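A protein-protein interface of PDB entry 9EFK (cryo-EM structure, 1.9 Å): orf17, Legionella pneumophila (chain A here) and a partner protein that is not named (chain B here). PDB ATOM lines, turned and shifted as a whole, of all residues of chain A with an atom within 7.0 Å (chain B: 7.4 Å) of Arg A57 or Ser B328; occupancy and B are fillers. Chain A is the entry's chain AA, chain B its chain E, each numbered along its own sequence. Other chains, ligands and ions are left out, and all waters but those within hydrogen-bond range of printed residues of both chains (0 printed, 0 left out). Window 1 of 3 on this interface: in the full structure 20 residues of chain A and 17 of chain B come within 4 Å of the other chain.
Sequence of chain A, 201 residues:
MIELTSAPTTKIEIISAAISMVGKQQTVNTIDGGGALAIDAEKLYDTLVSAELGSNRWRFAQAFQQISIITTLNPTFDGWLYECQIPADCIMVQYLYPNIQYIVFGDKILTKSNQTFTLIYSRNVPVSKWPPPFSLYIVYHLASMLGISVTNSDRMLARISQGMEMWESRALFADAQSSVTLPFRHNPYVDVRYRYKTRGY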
ATOM      1  N   GLU A  52     -10.573  29.092  -6.203  1.00  0.00           N
ATOM      2  CA  GLU A  52     -11.260  27.842  -5.911  1.00  0.00           C
ATOM      3  C   GLU A  52     -12.676  28.092  -5.413  1.00  0.00           C
ATOM      4  O   GLU A  52     -13.626  27.439  -5.858  1.00  0.00           O
ATOM      5  CB  GLU A  52     -10.455  27.046  -4.887  1.00  0.00           C
ATOM      6  CG  GLU A  52     -10.276  25.604  -5.254  1.00  0.00           C
ATOM      7  CD  GLU A  52     -11.584  24.870  -5.285  1.00  0.00           C
ATOM      8  OE1 GLU A  52     -12.438  25.180  -4.442  1.00  0.00           O
ATOM      9  OE2 GLU A  52     -11.763  23.995  -6.147  1.00  0.00           O
ATOM     10  N   LEU A  53     -12.841  29.040  -4.493  1.00  0.00           N
ATOM     11  CA  LEU A  53     -14.168  29.349  -3.982  1.00  0.00           C
ATOM     12  C   LEU A  53     -15.014  30.103  -4.998  1.00  0.00           C
ATOM     13  O   LEU A  53     -16.240  30.103  -4.882  1.00  0.00           O
ATOM     14  CB  LEU A  53     -14.056  30.153  -2.687  1.00  0.00           C
ATOM     15  CG  LEU A  53     -13.357  29.445  -1.526  1.00  0.00           C
ATOM     16  CD1 LEU A  53     -13.241  30.356  -0.326  1.00  0.00           C
ATOM     17  CD2 LEU A  53     -14.090  28.176  -1.160  1.00  0.00           C
ATOM     18  N   GLY A  54     -14.394  30.725  -5.991  1.00  0.00           N
ATOM     19  CA  GLY A  54     -15.093  31.463  -7.014  1.00  0.00           C
ATOM     20  C   GLY A  54     -15.452  30.691  -8.262  1.00  0.00           C
ATOM     21  O   GLY A  54     -15.935  31.296  -9.223  1.00  0.00           O
ATOM     22  N   SER A  55     -15.238  29.378  -8.291  1.00  0.00           N
ATOM     23  CA  SER A  55     -15.501  28.606  -9.496  1.00  0.00           C
ATOM     24  C   SER A  55     -16.367  27.379  -9.242  1.00  0.00           C
ATOM     25  O   SER A  55     -16.539  26.564 -10.151  1.00  0.00           O
ATOM     26  CB  SER A  55     -14.187  28.187 -10.160  1.00  0.00           C
ATOM     27  OG  SER A  55     -13.366  27.469  -9.262  1.00  0.00           O
ATOM     28  N   ASN A  56     -16.916  27.231  -8.043  1.00  0.00           N
ATOM     29  CA  ASN A  56     -17.723  26.070  -7.709  1.00  0.00           C
ATOM     30  C   ASN A  56     -18.634  26.433  -6.549  1.00  0.00           C
ATOM     31  O   ASN A  56     -18.279  27.252  -5.701  1.00  0.00           O
ATOM     32  CB  ASN A  56     -16.842  24.870  -7.351  1.00  0.00           C
ATOM     33  CG  ASN A  56     -17.645  23.657  -6.964  1.00  0.00           C
ATOM     34  OD1 ASN A  56     -18.151  22.941  -7.819  1.00  0.00           O
ATOM     35  ND2 ASN A  56     -17.769  23.419  -5.669  1.00  0.00           N
ATOM     36  N   ARG A  57     -19.809  25.815  -6.518  1.00  0.00           N
ATOM     37  CA  ARG A  57     -20.749  26.038  -5.424  1.00  0.00           C
ATOM     38  C   ARG A  57     -20.354  25.139  -4.263  1.00  0.00           C
ATOM     39  O   ARG A  57     -20.775  23.989  -4.164  1.00  0.00           O
ATOM     40  CB  ARG A  57     -22.181  25.774  -5.865  1.00  0.00           C
ATOM     41  CG  ARG A  57     -23.213  26.127  -4.807  1.00  0.00           C
ATOM     42  CD  ARG A  57     -24.240  25.027  -4.634  1.00  0.00           C
ATOM     43  NE  ARG A  57     -23.636  23.789  -4.161  1.00  0.00           N
ATOM     44  CZ  ARG A  57     -24.267  22.626  -4.092  1.00  0.00           C
ATOM     45  NH1 ARG A  57     -25.532  22.506  -4.450  1.00  0.00           N
ATOM     46  NH2 ARG A  57     -23.610  21.557  -3.657  1.00  0.00           N
ATOM     47  N   TRP A  58     -19.513  25.666  -3.382  1.00  0.00           N
ATOM     48  CA  TRP A  58     -19.253  25.040  -2.096  1.00  0.00           C
ATOM     49  C   TRP A  58     -20.300  25.530  -1.108  1.00  0.00           C
ATOM     50  O   TRP A  58     -20.521  26.736  -0.988  1.00  0.00           O
ATOM     51  CB  TRP A  58     -17.853  25.379  -1.589  1.00  0.00           C
ATOM     52  CG  TRP A  58     -16.742  24.881  -2.444  1.00  0.00           C
ATOM     53  CD1 TRP A  58     -16.118  25.555  -3.445  1.00  0.00           C
ATOM     54  CD2 TRP A  58     -16.106  23.606  -2.360  1.00  0.00           C
ATOM     55  NE1 TRP A  58     -15.139  24.777  -3.998  1.00  0.00           N
ATOM     56  CE2 TRP A  58     -15.110  23.573  -3.347  1.00  0.00           C
ATOM     57  CE3 TRP A  58     -16.287  22.485  -1.546  1.00  0.00           C
ATOM     58  CZ2 TRP A  58     -14.297  22.466  -3.545  1.00  0.00           C
ATOM     59  CZ3 TRP A  58     -15.481  21.392  -1.743  1.00  0.00           C
ATOM     60  CH2 TRP A  58     -14.495  21.390  -2.731  1.00  0.00           C
ATOM     61  N   ARG A  59     -20.949  24.597  -0.412  1.00  0.00           N
ATOM     62  CA  ARG A  59     -21.996  24.988   0.525  1.00  0.00           C
ATOM     63  C   ARG A  59     -21.446  25.876   1.629  1.00  0.00           C
ATOM     64  O   ARG A  59     -22.090  26.850   2.027  1.00  0.00           O
ATOM     65  CB  ARG A  59     -22.669  23.757   1.125  1.00  0.00           C
ATOM     66  CG  ARG A  59     -23.437  22.910   0.142  1.00  0.00           C
ATOM     67  CD  ARG A  59     -24.353  21.955   0.874  1.00  0.00           C
ATOM     68  NE  ARG A  59     -24.793  20.848   0.037  1.00  0.00           N
ATOM     69  CZ  ARG A  59     -25.800  20.910  -0.820  1.00  0.00           C
ATOM     70  NH1 ARG A  59     -26.485  22.026  -1.000  1.00  0.00           N
ATOM     71  NH2 ARG A  59     -26.127  19.828  -1.516  1.00  0.00           N
ATOM     72  N   PHE A  60     -20.255  25.561   2.137  1.00  0.00           N
ATOM     73  CA  PHE A  60     -19.714  26.331   3.249  1.00  0.00           C
ATOM     74  C   PHE A  60     -19.319  27.744   2.842  1.00  0.00           C
ATOM     75  O   PHE A  60     -19.146  28.596   3.715  1.00  0.00           O
ATOM     76  CB  PHE A  60     -18.519  25.605   3.873  1.00  0.00           C
ATOM     77  CG  PHE A  60     -17.295  25.570   3.008  1.00  0.00           C
ATOM     78  CD1 PHE A  60     -17.102  24.545   2.106  1.00  0.00           C
ATOM     79  CD2 PHE A  60     -16.319  26.544   3.119  1.00  0.00           C
ATOM     80  CE1 PHE A  60     -15.975  24.501   1.324  1.00  0.00           C
ATOM     81  CE2 PHE A  60     -15.191  26.505   2.337  1.00  0.00           C
ATOM     82  CZ  PHE A  60     -15.020  25.483   1.436  1.00  0.00           C
ATOM     83  N   ALA A  61     -19.170  28.013   1.548  1.00  0.00           N
ATOM     84  CA  ALA A  61     -18.791  29.332   1.067  1.00  0.00           C
ATOM     85  C   ALA A  61     -19.970  30.138   0.541  1.00  0.00           C
ATOM     86  O   ALA A  61     -19.769  31.233   0.015  1.00  0.00           O
ATOM     87  CB  ALA A  61     -17.722  29.207  -0.017  1.00  0.00           C
ATOM     88  N   GLN A  62     -21.191  29.632   0.671  1.00  0.00           N
ATOM     89  CA  GLN A  62     -22.357  30.347   0.178  1.00  0.00           C
ATOM     90  C   GLN A  62     -22.769  31.464   1.128  1.00  0.00           C
ATOM     91  O   GLN A  62     -22.540  31.399   2.336  1.00  0.00           O
ATOM     92  CB  GLN A  62     -23.528  29.392  -0.026  1.00  0.00           C
ATOM     93  CG  GLN A  62     -23.415  28.557  -1.272  1.00  0.00           C
ATOM     94  CD  GLN A  62     -24.620  27.682  -1.485  1.00  0.00           C
ATOM     95  OE1 GLN A  62     -24.860  26.750  -0.727  1.00  0.00           O
ATOM     96  NE2 GLN A  62     -25.389  27.976  -2.522  1.00  0.00           N
ATOM     97  N   MET A  92     -18.692  34.914  -6.807  1.00  0.00           N
ATOM     98  CA  MET A  92     -19.321  34.212  -7.922  1.00  0.00           C
ATOM     99  C   MET A  92     -20.826  34.292  -7.745  1.00  0.00           C
ATOM    100  O   MET A  92     -21.356  33.773  -6.763  1.00  0.00           O
ATOM    101  CB  MET A  92     -18.871  32.754  -7.995  1.00  0.00           C
ATOM    102  CG  MET A  92     -19.515  31.984  -9.135  1.00  0.00           C
ATOM    103  SD  MET A  92     -19.079  30.239  -9.225  1.00  0.00           S
ATOM    104  CE  MET A  92     -19.896  29.615  -7.773  1.00  0.00           C
ATOM    105  N   GLN A  94     -24.468  33.134  -8.170  1.00  0.00           N
ATOM    106  CA  GLN A  94     -25.072  31.825  -8.369  1.00  0.00           C
ATOM    107  C   GLN A  94     -26.517  31.919  -8.842  1.00  0.00           C
ATOM    108  O   GLN A  94     -26.842  31.384  -9.903  1.00  0.00           O
ATOM    109  CB  GLN A  94     -24.964  31.001  -7.086  1.00  0.00           C
ATOM    110  CG  GLN A  94     -23.535  30.647  -6.756  1.00  0.00           C
ATOM    111  CD  GLN A  94     -23.393  29.931  -5.443  1.00  0.00           C
ATOM    112  OE1 GLN A  94     -24.375  29.495  -4.855  1.00  0.00           O
ATOM    113  NE2 GLN A  94     -22.167  29.809  -4.971  1.00  0.00           N
ATOM    114  N   TYR A  95     -27.394  32.595  -8.107  1.00  0.00           N
ATOM    115  CA  TYR A  95     -28.756  32.798  -8.586  1.00  0.00           C
ATOM    116  C   TYR A  95     -29.431  33.872  -7.747  1.00  0.00           C
ATOM    117  O   TYR A  95     -28.887  34.347  -6.750  1.00  0.00           O
ATOM    118  CB  TYR A  95     -29.569  31.501  -8.573  1.00  0.00           C
ATOM    119  CG  TYR A  95     -29.868  30.933  -7.210  1.00  0.00           C
ATOM    120  CD1 TYR A  95     -28.962  30.109  -6.566  1.00  0.00           C
ATOM    121  CD2 TYR A  95     -31.072  31.198  -6.582  1.00  0.00           C
ATOM    122  CE1 TYR A  95     -29.243  29.579  -5.333  1.00  0.00           C
ATOM    123  CE2 TYR A  95     -31.357  30.679  -5.350  1.00  0.00           C
ATOM    124  CZ  TYR A  95     -30.442  29.870  -4.730  1.00  0.00           C
ATOM    125  OH  TYR A  95     -30.731  29.347  -3.497  1.00  0.00           O
ATOM    126  N   SER A 122     -21.221  33.145  -3.871  1.00  0.00           N
ATOM    127  CA  SER A 122     -20.090  32.561  -3.175  1.00  0.00           C
ATOM    128  C   SER A 122     -19.182  33.672  -2.668  1.00  0.00           C
ATOM    129  O   SER A 122     -19.038  34.715  -3.305  1.00  0.00           O
ATOM    130  CB  SER A 122     -19.310  31.627  -4.099  1.00  0.00           C
ATOM    131  OG  SER A 122     -18.428  30.809  -3.361  1.00  0.00           O
ATOM    132  N   LEU A 172     -15.472  17.571  -2.372  1.00  0.00           N
ATOM    133  CA  LEU A 172     -16.713  17.902  -3.065  1.00  0.00           C
ATOM    134  C   LEU A 172     -17.850  16.991  -2.632  1.00  0.00           C
ATOM    135  O   LEU A 172     -18.978  17.450  -2.437  1.00  0.00           O
ATOM    136  CB  LEU A 172     -16.514  17.819  -4.575  1.00  0.00           C
ATOM    137  CG  LEU A 172     -15.834  19.013  -5.237  1.00  0.00           C
ATOM    138  CD1 LEU A 172     -15.407  18.664  -6.642  1.00  0.00           C
ATOM    139  CD2 LEU A 172     -16.765  20.201  -5.241  1.00  0.00           C
ATOM    140  N   ASP A 175     -18.960  17.847   0.988  1.00  0.00           N
ATOM    141  CA  ASP A 175     -19.737  19.079   0.990  1.00  0.00           C
ATOM    142  C   ASP A 175     -21.131  18.863   0.413  1.00  0.00           C
ATOM    143  O   ASP A 175     -22.115  19.383   0.945  1.00  0.00           O
ATOM    144  CB  ASP A 175     -18.989  20.158   0.210  1.00  0.00           C
ATOM    145  CG  ASP A 175     -19.746  21.461   0.144  1.00  0.00           C
ATOM    146  OD1 ASP A 175     -19.755  22.193   1.150  1.00  0.00           O
ATOM    147  OD2 ASP A 175     -20.322  21.761  -0.920  1.00  0.00           O
ATOM    148  N   ALA A 176     -21.238  18.085  -0.663  1.00  0.00           N
ATOM    149  CA  ALA A 176     -22.494  17.983  -1.394  1.00  0.00           C
ATOM    150  C   ALA A 176     -23.503  17.047  -0.742  1.00  0.00           C
ATOM    151  O   ALA A 176     -24.706  17.304  -0.820  1.00  0.00           O
ATOM    152  CB  ALA A 176     -22.229  17.523  -2.823  1.00  0.00           C
ATOM    153  N   GLN A 177     -23.051  15.961  -0.115  1.00  0.00           N
ATOM    154  CA  GLN A 177     -23.976  14.919   0.319  1.00  0.00           C
ATOM    155  C   GLN A 177     -24.825  15.319   1.517  1.00  0.00           C
ATOM    156  O   GLN A 177     -25.789  14.616   1.824  1.00  0.00           O
ATOM    157  CB  GLN A 177     -23.218  13.625   0.634  1.00  0.00           C
ATOM    158  CG  GLN A 177     -22.068  13.761   1.615  1.00  0.00           C
ATOM    159  CD  GLN A 177     -22.518  13.913   3.043  1.00  0.00           C
ATOM    160  OE1 GLN A 177     -23.355  13.158   3.521  1.00  0.00           O
ATOM    161  NE2 GLN A 177     -21.980  14.904   3.729  1.00  0.00           N
ATOM    162  N   VAL A 180     -30.166  17.711   0.208  1.00  0.00           N
ATOM    163  CA  VAL A 180     -30.821  17.166  -0.972  1.00  0.00           C
ATOM    164  C   VAL A 180     -30.477  18.003  -2.199  1.00  0.00           C
ATOM    165  O   VAL A 180     -30.011  19.143  -2.108  1.00  0.00           O
ATOM    166  CB  VAL A 180     -32.342  17.089  -0.768  1.00  0.00           C
ATOM    167  CG1 VAL A 180     -32.668  16.241   0.440  1.00  0.00           C
ATOM    168  CG2 VAL A 180     -32.927  18.480  -0.628  1.00  0.00           C
ATOM    169  N   THR A 181     -30.709  17.419  -3.369  1.00  0.00           N
ATOM    170  CA  THR A 181     -30.516  18.130  -4.623  1.00  0.00           C
ATOM    171  C   THR A 181     -31.754  18.959  -4.931  1.00  0.00           C
ATOM    172  O   THR A 181     -32.879  18.458  -4.868  1.00  0.00           O
ATOM    173  CB  THR A 181     -30.237  17.150  -5.762  1.00  0.00           C
ATOM    174  OG1 THR A 181     -29.089  16.358  -5.443  1.00  0.00           O
ATOM    175  CG2 THR A 181     -29.978  17.898  -7.057  1.00  0.00           C
ATOM    176  N   LEU A 182     -31.548  20.226  -5.239  1.00  0.00           N
ATOM    177  CA  LEU A 182     -32.654  21.113  -5.558  1.00  0.00           C
ATOM    178  C   LEU A 182     -33.149  20.875  -6.983  1.00  0.00           C
ATOM    179  O   LEU A 182     -32.370  20.514  -7.866  1.00  0.00           O
ATOM    180  CB  LEU A 182     -32.229  22.566  -5.396  1.00  0.00           C
ATOM    181  CG  LEU A 182     -31.813  22.967  -3.982  1.00  0.00           C
ATOM    182  CD1 LEU A 182     -31.394  24.422  -3.943  1.00  0.00           C
ATOM    183  CD2 LEU A 182     -32.937  22.707  -3.001  1.00  0.00           C
ATOM    184  N   ALA B 324     -22.020  12.182  -9.714  1.00  0.00           N
ATOM    185  CA  ALA B 324     -20.868  13.066  -9.775  1.00  0.00           C
ATOM    186  C   ALA B 324     -20.286  13.175  -8.378  1.00  0.00           C
ATOM    187  O   ALA B 324     -20.851  12.668  -7.409  1.00  0.00           O
ATOM    188  CB  ALA B 324     -21.244  14.443 -10.328  1.00  0.00           C
ATOM    189  N   ALA B 325     -19.138  13.840  -8.288  1.00  0.00           N
ATOM    190  CA  ALA B 325     -18.583  14.159  -6.981  1.00  0.00           C
ATOM    191  C   ALA B 325     -19.505  15.083  -6.201  1.00  0.00           C
ATOM    192  O   ALA B 325     -19.611  14.965  -4.978  1.00  0.00           O
ATOM    193  CB  ALA B 325     -17.198  14.784  -7.135  1.00  0.00           C
ATOM    194  N   SER B 326     -20.185  15.999  -6.882  1.00  0.00           N
ATOM    195  CA  SER B 326     -21.051  16.954  -6.213  1.00  0.00           C
ATOM    196  C   SER B 326     -22.205  17.318  -7.130  1.00  0.00           C
ATOM    197  O   SER B 326     -22.070  17.303  -8.353  1.00  0.00           O
ATOM    198  CB  SER B 326     -20.274  18.212  -5.807  1.00  0.00           C
ATOM    199  OG  SER B 326     -21.138  19.216  -5.316  1.00  0.00           O
ATOM    200  N   ASP B 327     -23.342  17.661  -6.527  1.00  0.00           N
ATOM    201  CA  ASP B 327     -24.465  18.175  -7.300  1.00  0.00           C
ATOM    202  C   ASP B 327     -24.218  19.579  -7.827  1.00  0.00           C
ATOM    203  O   ASP B 327     -25.089  20.132  -8.503  1.00  0.00           O
ATOM    204  CB  ASP B 327     -25.750  18.151  -6.472  1.00  0.00           C
ATOM    205  CG  ASP B 327     -25.684  19.048  -5.252  1.00  0.00           C
ATOM    206  OD1 ASP B 327     -24.703  18.964  -4.491  1.00  0.00           O
ATOM    207  OD2 ASP B 327     -26.626  19.840  -5.052  1.00  0.00           O
ATOM    208  N   SER B 328     -23.067  20.168  -7.533  1.00  0.00           N
ATOM    209  CA  SER B 328     -22.671  21.444  -8.102  1.00  0.00           C
ATOM    210  C   SER B 328     -22.069  21.306  -9.493  1.00  0.00           C
ATOM    211  O   SER B 328     -21.466  22.262  -9.982  1.00  0.00           O
ATOM    212  CB  SER B 328     -21.671  22.139  -7.179  1.00  0.00           C
ATOM    213  OG  SER B 328     -20.442  21.443  -7.157  1.00  0.00           O
ATOM    214  N   ALA B 329     -22.220  20.146 -10.137  1.00  0.00           N
ATOM    215  CA  ALA B 329     -21.671  19.967 -11.476  1.00  0.00           C
ATOM    216  C   ALA B 329     -22.311  20.918 -12.476  1.00  0.00           C
ATOM    217  O   ALA B 329     -21.646  21.364 -13.414  1.00  0.00           O
ATOM    218  CB  ALA B 329     -21.836  18.521 -11.930  1.00  0.00           C
ATOM    219  N   PHE B 330     -23.593  21.228 -12.312  1.00  0.00           N
ATOM    220  CA  PHE B 330     -24.196  22.340 -13.030  1.00  0.00           C
ATOM    221  C   PHE B 330     -25.128  23.095 -12.092  1.00  0.00           C
ATOM    222  O   PHE B 330     -25.471  22.626 -11.008  1.00  0.00           O
ATOM    223  CB  PHE B 330     -24.927  21.893 -14.307  1.00  0.00           C
ATOM    224  CG  PHE B 330     -25.863  20.729 -14.126  1.00  0.00           C
ATOM    225  CD1 PHE B 330     -27.032  20.855 -13.401  1.00  0.00           C
ATOM    226  CD2 PHE B 330     -25.595  19.523 -14.745  1.00  0.00           C
ATOM    227  CE1 PHE B 330     -27.892  19.789 -13.263  1.00  0.00           C
ATOM    228  CE2 PHE B 330     -26.455  18.457 -14.615  1.00  0.00           C
ATOM    229  CZ  PHE B 330     -27.605  18.591 -13.874  1.00  0.00           C
ATOM    230  N   ASN B 331     -25.508  24.294 -12.514  1.00  0.00           N
ATOM    231  CA  ASN B 331     -26.353  25.180 -11.723  1.00  0.00           C
ATOM    232  C   ASN B 331     -27.812  24.828 -11.987  1.00  0.00           C
ATOM    233  O   ASN B 331     -28.329  25.087 -13.076  1.00  0.00           O
ATOM    234  CB  ASN B 331     -26.053  26.633 -12.085  1.00  0.00           C
ATOM    235  CG  ASN B 331     -26.686  27.624 -11.138  1.00  0.00           C
ATOM    236  OD1 ASN B 331     -27.724  27.364 -10.545  1.00  0.00           O
ATOM    237  ND2 ASN B 331     -26.063  28.783 -11.006  1.00  0.00           N
ATOM    238  N   GLN B 332     -28.481  24.245 -10.990  1.00  0.00           N
ATOM    239  CA  GLN B 332     -29.878  23.854 -11.162  1.00  0.00           C
ATOM    240  C   GLN B 332     -30.790  25.058 -11.361  1.00  0.00           C
ATOM    241  O   GLN B 332     -31.841  24.933 -11.993  1.00  0.00           O
ATOM    242  CB  GLN B 332     -30.363  23.037  -9.965  1.00  0.00           C
ATOM    243  CG  GLN B 332     -29.870  21.604  -9.918  1.00  0.00           C
ATOM    244  CD  GLN B 332     -28.445  21.488  -9.427  1.00  0.00           C
ATOM    245  OE1 GLN B 332     -27.921  22.394  -8.789  1.00  0.00           O
ATOM    246  NE2 GLN B 332     -27.811  20.366  -9.723  1.00  0.00           N
ATOM    247  N   GLN B 333     -30.420  26.217 -10.819  1.00  0.00           N
ATOM    248  CA  GLN B 333     -31.289  27.387 -10.883  1.00  0.00           C
ATOM    249  C   GLN B 333     -31.268  28.056 -12.246  1.00  0.00           C
ATOM    250  O   GLN B 333     -32.283  28.620 -12.664  1.00  0.00           O
ATOM    251  CB  GLN B 333     -30.889  28.399  -9.816  1.00  0.00           C
ATOM    252  CG  GLN B 333     -30.344  27.772  -8.565  1.00  0.00           C
ATOM    253  CD  GLN B 333     -31.374  26.966  -7.836  1.00  0.00           C
ATOM    254  OE1 GLN B 333     -32.566  27.250  -7.913  1.00  0.00           O
ATOM    255  NE2 GLN B 333     -30.928  25.943  -7.122  1.00  0.00           N
ATOM    256  N   PRO B 344     -23.709  24.918 -19.143  1.00  0.00           N
ATOM    257  CA  PRO B 344     -22.361  24.841 -18.564  1.00  0.00           C
ATOM    258  C   PRO B 344     -22.305  23.717 -17.540  1.00  0.00           C
ATOM    259  O   PRO B 344     -23.103  23.680 -16.603  1.00  0.00           O
ATOM    260  CB  PRO B 344     -22.173  26.216 -17.912  1.00  0.00           C
ATOM    261  CG  PRO B 344     -23.231  27.077 -18.502  1.00  0.00           C
ATOM    262  CD  PRO B 344     -24.375  26.183 -18.808  1.00  0.00           C
ATOM    263  N   VAL B 345     -21.380  22.783 -17.737  1.00  0.00           N
ATOM    264  CA  VAL B 345     -21.263  21.609 -16.883  1.00  0.00           C
ATOM    265  C   VAL B 345     -19.797  21.381 -16.557  1.00  0.00           C
ATOM    266  O   VAL B 345     -18.953  21.360 -17.457  1.00  0.00           O
ATOM    267  CB  VAL B 345     -21.860  20.352 -17.548  1.00  0.00           C
ATOM    268  CG1 VAL B 345     -21.611  19.136 -16.692  1.00  0.00           C
ATOM    269  CG2 VAL B 345     -23.340  20.528 -17.793  1.00  0.00           C
ATOM    270  N   GLN B 346     -19.490  21.200 -15.277  1.00  0.00           N
ATOM    271  CA  GLN B 346     -18.165  20.739 -14.872  1.00  0.00           C
ATOM    272  C   GLN B 346     -18.064  19.262 -15.214  1.00  0.00           C
ATOM    273  O   GLN B 346     -18.501  18.403 -14.448  1.00  0.00           O
ATOM    274  CB  GLN B 346     -17.935  20.980 -13.386  1.00  0.00           C
ATOM    275  CG  GLN B 346     -18.141  22.409 -12.951  1.00  0.00           C
ATOM    276  CD  GLN B 346     -17.772  22.627 -11.504  1.00  0.00           C
ATOM    277  OE1 GLN B 346     -16.631  22.414 -11.109  1.00  0.00           O
ATOM    278  NE2 GLN B 346     -18.737  23.044 -10.703  1.00  0.00           N
ATOM    279  N   GLN B 349     -14.813  16.439 -12.142  1.00  0.00           N
ATOM    280  CA  GLN B 349     -14.602  17.025 -10.819  1.00  0.00           C
ATOM    281  C   GLN B 349     -13.609  16.146 -10.069  1.00  0.00           C
ATOM    282  O   GLN B 349     -13.968  15.076  -9.571  1.00  0.00           O
ATOM    283  CB  GLN B 349     -15.917  17.162 -10.061  1.00  0.00           C
ATOM    284  CG  GLN B 349     -16.779  18.306 -10.540  1.00  0.00           C
ATOM    285  CD  GLN B 349     -18.094  18.401  -9.804  1.00  0.00           C
ATOM    286  OE1 GLN B 349     -18.792  17.408  -9.623  1.00  0.00           O
ATOM    287  NE2 GLN B 349     -18.440  19.602  -9.373  1.00  0.00           N
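Of the 22 printed residues of chain A, 9 touch a printed residue of chain B.
Printed residues of chain A that touch a printed residue of chain B: Asn A56, Arg A57, Arg A59, Gln A94, Tyr A95, Leu A172, Ala A176, Thr A181 and Leu A182.
Of the 14 printed residues of chain B, 9 touch a printed residue of chain A.
Printed residues of chain B that touch a printed residue of chain A: Ala B325, Ser B326, Asp B327, Ser B328, Asn B331, Gln B332, Gln B333, Gln B346 and Gln B349.
Along chain B the printed residues that touch a printed residue of chain A span positions 325 to 349.
O of Ala B329 is in hydrogen-bond range of N of Gln B346.
OD1 of Asn B331 lies within hydrogen-bond range of N of Gln B333 (2.9 Å).
ND2 of Asn A56 sits close to NE1 of Trp A58, 3.4 Å away.
OD2 of Asp A175 lies within hydrogen-bond range of N of Arg A59.
NH2 of Arg A59 lies within hydrogen-bond range of O of Ala A176 (3.0 Å).
The side-chain amide nitrogen (NE2) of Gln A62 is in hydrogen-bond range of the side-chain amide oxygen (OE1) of Gln A94 (3.0 Å).
Among the printed residues, pairs that only touch across the chains: Asn A56 with Gln B349 (3.7 Å), Arg A57 with Ser B326 (3.8 Å), Arg A57 with Ser B328 (3.6 Å), Tyr A95 with Gln B333 (3.4 Å), Leu A172 with Ala B325 (3.6 Å), Leu A172 with Ser B326 (3.7 Å), Leu A172 with Gln B349 (3.8 Å), Ala A176 with Ser B326 (3.2 Å), Ala A176 with Asp B327 (3.3 Å), Thr A181 with Asp B327 (3.9 Å), Leu A182 with Gln B332 (3.4 Å) and Leu A182 with Gln B333 (3.6 Å).
Of the printed residues of chain B, Asn A56 touches Ser B328 (2.8 Å), Gln B346 (2.9 Å) and Gln B349 (3.7 Å).
Arg A57 touches just these residues of chain B: Ser B326 (3.8 Å), Asp B327 (2.9 Å) and Ser B328 (3.6 Å).
Of the printed residues of chain B, Arg A59 touches Asp B327 (3.4 Å).
Of the printed residues of chain B, Leu A172 touches Ala B325 (3.6 Å), Ser B326 (3.7 Å) and Gln B349 (3.8 Å).
Of the printed residues of chain B, Thr A181 touches Asp B327.
The nearest residue of chain A that does not touch Ser B328 is Leu A172 (4.3 Å).
The nearest printed residue of chain B that does not touch Arg A59 is Ser B326 (6.3 Å).
The side-chain carboxylate (OD1) of Asp B327 is in salt-bridge range of the guanidinium group (NH2) of Arg A57.
The side-chain carboxylate (OD1) of Asp B327 is in salt-bridge range of the guanidinium group (NH2) of Arg A59, 3.4 Å away.
The side-chain amide oxygen (OD1) of Asn A56 is in hydrogen-bond range of the side-chain hydroxyl (OG) of Ser B328, 2.8 Å away.
The side-chain amide nitrogen of Asn B331 sits at hydrogen-bond distance from the backbone carbonyl oxygen of Gln A94 (2.9 Å).
NE2 of Gln B346 is in hydrogen-bond range of OD1 of Asn A56 (2.9 Å).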
